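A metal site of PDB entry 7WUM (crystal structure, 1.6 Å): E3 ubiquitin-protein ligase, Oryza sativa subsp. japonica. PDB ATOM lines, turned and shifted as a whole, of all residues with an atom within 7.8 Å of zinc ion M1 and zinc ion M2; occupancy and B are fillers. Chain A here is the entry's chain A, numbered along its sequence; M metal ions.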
ATOM      1  N   ALA A   1       1.956  -9.736  13.980  1.00  0.00           N
ATOM      2  CA  ALA A   1       2.853 -10.718  14.627  1.00  0.00           C
ATOM      3  C   ALA A   1       3.370 -11.748  13.610  1.00  0.00           C
ATOM      4  O   ALA A   1       4.585 -11.860  13.480  1.00  0.00           O
ATOM      5  CB  ALA A   1       2.150 -11.375  15.779  1.00  0.00           C
ATOM      6  N   VAL A   2       2.465 -12.507  12.986  1.00  0.00           N
ATOM      7  CA  VAL A   2       2.859 -13.482  11.933  1.00  0.00           C
ATOM      8  C   VAL A   2       2.210 -13.029  10.628  1.00  0.00           C
ATOM      9  O   VAL A   2       1.018 -12.762  10.621  1.00  0.00           O
ATOM     10  CB  VAL A   2       2.468 -14.939  12.282  1.00  0.00           C
ATOM     11  CG1 VAL A   2       2.660 -15.879  11.099  1.00  0.00           C
ATOM     12  CG2 VAL A   2       3.216 -15.451  13.499  1.00  0.00           C
ATOM     13  N   CYS A   3       3.008 -12.953   9.577  1.00  0.00           N
ATOM     14  CA  CYS A   3       2.509 -12.493   8.266  1.00  0.00           C
ATOM     15  C   CYS A   3       1.298 -13.308   7.848  1.00  0.00           C
ATOM     16  O   CYS A   3       1.352 -14.534   7.893  1.00  0.00           O
ATOM     17  CB  CYS A   3       3.607 -12.623   7.229  1.00  0.00           C
ATOM     18  SG  CYS A   3       3.159 -11.898   5.633  1.00  0.00           S
ATOM     19  N   GLY A   4       0.255 -12.613   7.441  1.00  0.00           N
ATOM     20  CA  GLY A   4      -0.917 -13.304   6.935  1.00  0.00           C
ATOM     21  C   GLY A   4      -1.004 -13.379   5.424  1.00  0.00           C
ATOM     22  O   GLY A   4      -2.095 -13.560   4.876  1.00  0.00           O
ATOM     23  N   SER A   5       0.117 -13.246   4.728  1.00  0.00           N
ATOM     24  CA  SER A   5       0.114 -13.359   3.281  1.00  0.00           C
ATOM     25  C   SER A   5      -0.146 -14.793   2.854  1.00  0.00           C
ATOM     26  O   SER A   5       0.360 -15.747   3.455  1.00  0.00           O
ATOM     27  CB  SER A   5       1.434 -12.859   2.702  1.00  0.00           C
ATOM     28  OG  SER A   5       1.525 -11.444   2.739  1.00  0.00           O
ATOM     29  N   VAL A   6      -0.952 -14.951   1.810  1.00  0.00           N
ATOM     30  CA  VAL A   6      -1.187 -16.241   1.188  1.00  0.00           C
ATOM     31  C   VAL A   6      -0.936 -16.065  -0.299  1.00  0.00           C
ATOM     32  O   VAL A   6      -1.045 -14.968  -0.832  1.00  0.00           O
ATOM     33  CB  VAL A   6      -2.601 -16.758   1.458  1.00  0.00           C
ATOM     34  CG1 VAL A   6      -2.830 -16.936   2.941  1.00  0.00           C
ATOM     35  CG2 VAL A   6      -3.604 -15.800   0.877  1.00  0.00           C
ATOM     36  N   TRP A   7      -0.529 -17.153  -0.956  1.00  0.00           N
ATOM     37  CA  TRP A   7      -0.290 -17.090  -2.385  1.00  0.00           C
ATOM     38  C   TRP A   7      -0.660 -18.421  -3.036  1.00  0.00           C
ATOM     39  O   TRP A   7      -0.790 -19.446  -2.360  1.00  0.00           O
ATOM     40  CB  TRP A   7       1.168 -16.688  -2.715  1.00  0.00           C
ATOM     41  CG  TRP A   7       2.183 -17.657  -2.252  1.00  0.00           C
ATOM     42  CD1 TRP A   7       2.687 -18.711  -2.955  1.00  0.00           C
ATOM     43  CD2 TRP A   7       2.884 -17.644  -0.995  1.00  0.00           C
ATOM     44  NE1 TRP A   7       3.621 -19.388  -2.197  1.00  0.00           N
ATOM     45  CE2 TRP A   7       3.758 -18.738  -0.999  1.00  0.00           C
ATOM     46  CE3 TRP A   7       2.850 -16.819   0.132  1.00  0.00           C
ATOM     47  CZ2 TRP A   7       4.582 -19.039   0.079  1.00  0.00           C
ATOM     48  CZ3 TRP A   7       3.668 -17.121   1.197  1.00  0.00           C
ATOM     49  CH2 TRP A   7       4.528 -18.212   1.160  1.00  0.00           C
ATOM     50  N   ALA A  26       8.409 -21.321   3.900  1.00  0.00           N
ATOM     51  CA  ALA A  26       8.623 -20.295   2.875  1.00  0.00           C
ATOM     52  C   ALA A  26       8.096 -18.982   3.406  1.00  0.00           C
ATOM     53  O   ALA A  26       7.225 -18.931   4.283  1.00  0.00           O
ATOM     54  CB  ALA A  26       7.917 -20.648   1.564  1.00  0.00           C
ATOM     55  N   ILE A  27       8.621 -17.895   2.836  1.00  0.00           N
ATOM     56  CA  ILE A  27       8.135 -16.564   3.168  1.00  0.00           C
ATOM     57  C   ILE A  27       7.809 -15.817   1.883  1.00  0.00           C
ATOM     58  O   ILE A  27       8.371 -16.085   0.820  1.00  0.00           O
ATOM     59  CB  ILE A  27       9.125 -15.767   4.056  1.00  0.00           C
ATOM     60  CG1 ILE A  27      10.441 -15.472   3.346  1.00  0.00           C
ATOM     61  CG2 ILE A  27       9.314 -16.484   5.410  1.00  0.00           C
ATOM     62  CD1 ILE A  27      11.361 -14.582   4.158  1.00  0.00           C
ATOM     63  N   CYS A  28       6.879 -14.878   1.979  1.00  0.00           N
ATOM     64  CA  CYS A  28       6.441 -14.127   0.817  1.00  0.00           C
ATOM     65  C   CYS A  28       7.533 -13.184   0.332  1.00  0.00           C
ATOM     66  O   CYS A  28       8.458 -12.825   1.079  1.00  0.00           O
ATOM     67  CB  CYS A  28       5.147 -13.365   1.137  1.00  0.00           C
ATOM     68  SG  CYS A  28       5.320 -11.943   2.284  1.00  0.00           S
ATOM     69  N   VAL A  29       7.415 -12.741  -0.913  1.00  0.00           N
ATOM     70  CA  VAL A  29       8.442 -11.863  -1.486  1.00  0.00           C
ATOM     71  C   VAL A  29       8.629 -10.592  -0.653  1.00  0.00           C
ATOM     72  O   VAL A  29       9.784 -10.273  -0.320  1.00  0.00           O
ATOM     73  CB  VAL A  29       8.127 -11.572  -2.967  1.00  0.00           C
ATOM     74  CG1 VAL A  29       8.933 -10.378  -3.461  1.00  0.00           C
ATOM     75  CG2 VAL A  29       8.380 -12.809  -3.826  1.00  0.00           C
ATOM     76  N   PRO A  30       7.585  -9.829  -0.304  1.00  0.00           N
ATOM     77  CA  PRO A  30       7.844  -8.640   0.514  1.00  0.00           C
ATOM     78  C   PRO A  30       8.524  -8.941   1.836  1.00  0.00           C
ATOM     79  O   PRO A  30       9.374  -8.151   2.254  1.00  0.00           O
ATOM     80  CB  PRO A  30       6.457  -8.029   0.713  1.00  0.00           C
ATOM     81  CG  PRO A  30       5.577  -8.645  -0.290  1.00  0.00           C
ATOM     82  CD  PRO A  30       6.181  -9.927  -0.744  1.00  0.00           C
ATOM     83  N   CYS A  31       8.160 -10.029   2.513  1.00  0.00           N
ATOM     84  CA  CYS A  31       8.862 -10.356   3.754  1.00  0.00           C
ATOM     85  C   CYS A  31      10.329 -10.666   3.502  1.00  0.00           C
ATOM     86  O   CYS A  31      11.189 -10.318   4.332  1.00  0.00           O
ATOM     87  CB  CYS A  31       8.182 -11.532   4.469  1.00  0.00           C
ATOM     88  SG  CYS A  31       6.701 -11.011   5.334  1.00  0.00           S
ATOM     89  N   PHE A  32      10.643 -11.327   2.405  1.00  0.00           N
ATOM     90  CA  PHE A  32      12.048 -11.560   2.113  1.00  0.00           C
ATOM     91  C   PHE A  32      12.771 -10.257   1.837  1.00  0.00           C
ATOM     92  O   PHE A  32      13.876 -10.022   2.349  1.00  0.00           O
ATOM     93  CB  PHE A  32      12.201 -12.524   0.929  1.00  0.00           C
ATOM     94  CG  PHE A  32      13.618 -12.814   0.573  1.00  0.00           C
ATOM     95  CD1 PHE A  32      14.333 -11.948  -0.252  1.00  0.00           C
ATOM     96  CD2 PHE A  32      14.244 -13.912   1.100  1.00  0.00           C
ATOM     97  CE1 PHE A  32      15.684 -12.237  -0.565  1.00  0.00           C
ATOM     98  CE2 PHE A  32      15.573 -14.193   0.781  1.00  0.00           C
ATOM     99  CZ  PHE A  32      16.289 -13.339  -0.027  1.00  0.00           C
ATOM    100  N   ASN A  34      12.160  -7.310   2.852  1.00  0.00           N
ATOM    101  CA  ASN A  34      12.280  -6.471   4.025  1.00  0.00           C
ATOM    102  C   ASN A  34      13.031  -7.153   5.162  1.00  0.00           C
ATOM    103  O   ASN A  34      13.002  -6.660   6.301  1.00  0.00           O
ATOM    104  CB  ASN A  34      10.895  -6.011   4.485  1.00  0.00           C
ATOM    105  CG  ASN A  34      10.309  -4.949   3.588  1.00  0.00           C
ATOM    106  OD1 ASN A  34      11.042  -4.220   2.911  1.00  0.00           O
ATOM    107  ND2 ASN A  34       8.988  -4.855   3.567  1.00  0.00           N
ATOM    108  N   GLY A  35      13.709  -8.269   4.877  1.00  0.00           N
ATOM    109  CA  GLY A  35      14.557  -8.936   5.833  1.00  0.00           C
ATOM    110  C   GLY A  35      16.002  -8.988   5.359  1.00  0.00           C
ATOM    111  O   GLY A  35      16.364  -8.452   4.310  1.00  0.00           O
ATOM    112  N   CYS A  51       1.181 -20.242   2.858  1.00  0.00           N
ATOM    113  CA  CYS A  51       0.994 -19.151   3.792  1.00  0.00           C
ATOM    114  C   CYS A  51       2.350 -18.709   4.329  1.00  0.00           C
ATOM    115  O   CYS A  51       3.313 -19.524   4.549  1.00  0.00           O
ATOM    116  CB  CYS A  51       0.095 -19.549   4.958  1.00  0.00           C
ATOM    117  SG  CYS A  51      -1.598 -19.965   4.491  1.00  0.00           S
ATOM    118  N   CYS A  52       2.529 -17.425   4.524  1.00  0.00           N
ATOM    119  CA  CYS A  52       3.847 -16.932   4.892  1.00  0.00           C
ATOM    120  C   CYS A  52       4.220 -17.349   6.306  1.00  0.00           C
ATOM    121  O   CYS A  52       3.392 -17.302   7.225  1.00  0.00           O
ATOM    122  CB  CYS A  52       3.899 -15.420   4.732  1.00  0.00           C
ATOM    123  SG  CYS A  52       5.539 -14.738   5.009  1.00  0.00           S
ATOM    124  N   ASP A  53       5.474 -17.757   6.479  1.00  0.00           N
ATOM    125  CA  ASP A  53       5.978 -18.158   7.782  1.00  0.00           C
ATOM    126  C   ASP A  53       6.704 -17.037   8.515  1.00  0.00           C
ATOM    127  O   ASP A  53       7.229 -17.271   9.615  1.00  0.00           O
ATOM    128  CB  ASP A  53       6.924 -19.358   7.638  1.00  0.00           C
ATOM    129  CG  ASP A  53       6.184 -20.632   7.240  1.00  0.00           C
ATOM    130  OD1 ASP A  53       5.049 -20.844   7.687  1.00  0.00           O
ATOM    131  OD2 ASP A  53       6.751 -21.412   6.454  1.00  0.00           O
ATOM    132  N   CYS A  54       6.734 -15.828   7.962  1.00  0.00           N
ATOM    133  CA  CYS A  54       7.503 -14.771   8.597  1.00  0.00           C
ATOM    134  C   CYS A  54       6.831 -14.374   9.906  1.00  0.00           C
ATOM    135  O   CYS A  54       5.641 -14.042   9.932  1.00  0.00           O
ATOM    136  CB  CYS A  54       7.626 -13.566   7.667  1.00  0.00           C
ATOM    137  SG  CYS A  54       8.644 -12.250   8.316  1.00  0.00           S
ATOM    138  N   GLY A  55       7.597 -14.410  10.991  1.00  0.00           N
ATOM    139  CA  GLY A  55       7.074 -14.087  12.309  1.00  0.00           C
ATOM    140  C   GLY A  55       6.760 -15.295  13.155  1.00  0.00           C
ATOM    141  O   GLY A  55       6.573 -15.151  14.370  1.00  0.00           O
ATOM    142  N   GLY A  64      15.696 -14.207  10.654  1.00  0.00           N
ATOM    143  CA  GLY A  64      15.191 -14.129   9.310  1.00  0.00           C
ATOM    144  C   GLY A  64      13.849 -13.465   9.175  1.00  0.00           C
ATOM    145  O   GLY A  64      13.348 -13.368   8.051  1.00  0.00           O
ATOM    146  N   PHE A  65      13.258 -12.991  10.274  1.00  0.00           N
ATOM    147  CA  PHE A  65      12.009 -12.242  10.179  1.00  0.00           C
ATOM    148  C   PHE A  65      12.256 -10.892   9.523  1.00  0.00           C
ATOM    149  O   PHE A  65      13.280 -10.244   9.742  1.00  0.00           O
ATOM    150  CB  PHE A  65      11.402 -11.986  11.556  1.00  0.00           C
ATOM    151  CG  PHE A  65      10.953 -13.218  12.299  1.00  0.00           C
ATOM    152  CD1 PHE A  65      10.896 -14.460  11.683  1.00  0.00           C
ATOM    153  CD2 PHE A  65      10.537 -13.111  13.629  1.00  0.00           C
ATOM    154  CE1 PHE A  65      10.465 -15.577  12.382  1.00  0.00           C
ATOM    155  CE2 PHE A  65      10.112 -14.222  14.332  1.00  0.00           C
ATOM    156  CZ  PHE A  65      10.084 -15.459  13.717  1.00  0.00           C
ATOM    157  N   CYS A  66      11.279 -10.434   8.751  1.00  0.00           N
ATOM    158  CA  CYS A  66      11.380  -9.091   8.212  1.00  0.00           C
ATOM    159  C   CYS A  66      11.195  -8.051   9.318  1.00  0.00           C
ATOM    160  O   CYS A  66      10.851  -8.367  10.458  1.00  0.00           O
ATOM    161  CB  CYS A  66      10.359  -8.893   7.079  1.00  0.00           C
ATOM    162  SG  CYS A  66       8.692  -8.475   7.618  1.00  0.00           S
ATOM    163  N   SER A  67      11.456  -6.797   8.960  1.00  0.00           N
ATOM    164  CA  SER A  67      11.331  -5.695   9.909  1.00  0.00           C
ATOM    165  C   SER A  67       9.921  -5.531  10.457  1.00  0.00           C
ATOM    166  O   SER A  67       9.748  -5.028  11.567  1.00  0.00           O
ATOM    167  CB  SER A  67      11.818  -4.404   9.228  1.00  0.00           C
ATOM    168  OG  SER A  67      10.950  -4.022   8.173  1.00  0.00           O
ATOM    169  N   ARG A  68       8.913  -5.997   9.716  1.00  0.00           N
ATOM    170  CA  ARG A  68       7.510  -5.735  10.003  1.00  0.00           C
ATOM    171  C   ARG A  68       6.837  -6.845  10.812  1.00  0.00           C
ATOM    172  O   ARG A  68       5.685  -6.686  11.202  1.00  0.00           O
ATOM    173  CB  ARG A  68       6.756  -5.505   8.687  1.00  0.00           C
ATOM    174  CG  ARG A  68       7.422  -4.396   7.865  1.00  0.00           C
ATOM    175  CD  ARG A  68       6.740  -3.960   6.563  1.00  0.00           C
ATOM    176  NE  ARG A  68       5.365  -3.541   6.750  1.00  0.00           N
ATOM    177  CZ  ARG A  68       4.320  -4.356   6.685  1.00  0.00           C
ATOM    178  NH1 ARG A  68       4.445  -5.613   6.312  1.00  0.00           N
ATOM    179  NH2 ARG A  68       3.111  -3.879   6.971  1.00  0.00           N
ATOM    180  N   HIS A  69       7.533  -7.962  11.064  1.00  0.00           N
ATOM    181  CA  HIS A  69       6.982  -9.064  11.832  1.00  0.00           C
ATOM    182  C   HIS A  69       7.951  -9.534  12.890  1.00  0.00           C
ATOM    183  O   HIS A  69       7.685 -10.524  13.579  1.00  0.00           O
ATOM    184  CB  HIS A  69       6.600 -10.228  10.907  1.00  0.00           C
ATOM    185  CG  HIS A  69       5.587  -9.841   9.880  1.00  0.00           C
ATOM    186  ND1 HIS A  69       5.872  -9.806   8.526  1.00  0.00           N
ATOM    187  CD2 HIS A  69       4.321  -9.381  10.013  1.00  0.00           C
ATOM    188  CE1 HIS A  69       4.799  -9.398   7.873  1.00  0.00           C
ATOM    189  NE2 HIS A  69       3.852  -9.108   8.752  1.00  0.00           N
ATOM    190  N   LYS A  70       9.078  -8.846  13.044  1.00  0.00           N
ATOM    191  CA  LYS A  70      10.058  -9.127  14.086  1.00  0.00           C
ATOM    192  C   LYS A  70       9.457  -8.858  15.459  1.00  0.00           C
ATOM    193  O   LYS A  70       9.478  -7.722  15.942  1.00  0.00           O
ATOM    194  CB  LYS A  70      11.325  -8.294  13.864  1.00  0.00           C
ATOM    195  CG  LYS A  70      12.596  -9.104  14.025  1.00  0.00           C
ATOM    196  CD  LYS A  70      13.727  -8.566  13.158  1.00  0.00           C
ATOM    197  CE  LYS A  70      14.991  -9.412  13.294  1.00  0.00           C
ATOM    198  NZ  LYS A  70      15.743  -9.151  14.549  1.00  0.00           N
HETATM  199 ZN    ZN M   1       5.087 -12.475   4.571  1.00  0.00          ZN
HETATM  200 ZN    ZN M   2       7.481 -10.418   7.490  1.00  0.00          ZN
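The backbone NH (N) of Cys 52 lies within hydrogen-bond range of the backbone carbonyl oxygen (O) of Ser 5. SG of Cys 66 lies close to N of Arg 68, at 3.3 Å. SG of Cys 3 sits close to OG of Ser 5. O of Cys 54 is in hydrogen-bond range of N of Cys 3, 2.9 Å away. SG of Cys 52 lies close to N of Cys 54, 3.4 Å away.
The nearest printed residue that does not touch zinc ion M1 is Ser 5 (4.1 Å).
Within 4 Å of zinc ion M2: Cys 31, Cys 54, Cys 66 and His 69. The nearest printed residue that does not touch zinc ion M2 is Cys 3 (4.5 Å).
Zinc ion M1 is bound by the side-chain sulfur (SG) of Cys 3 (2.3 Å). SG of Cys 31 is bound to zinc ion M1 (2.3 Å). SG of Cys 52 binds zinc ion M1, 2.3 Å away. SG of Cys 28 is bound to zinc ion M1 (2.4 Å).
Zinc ion M2 is bound by ND1 of His 69, SG of Cys 66, SG of Cys 54 and SG of Cys 31. Zinc ion M2 has four donor atoms within binding distance.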
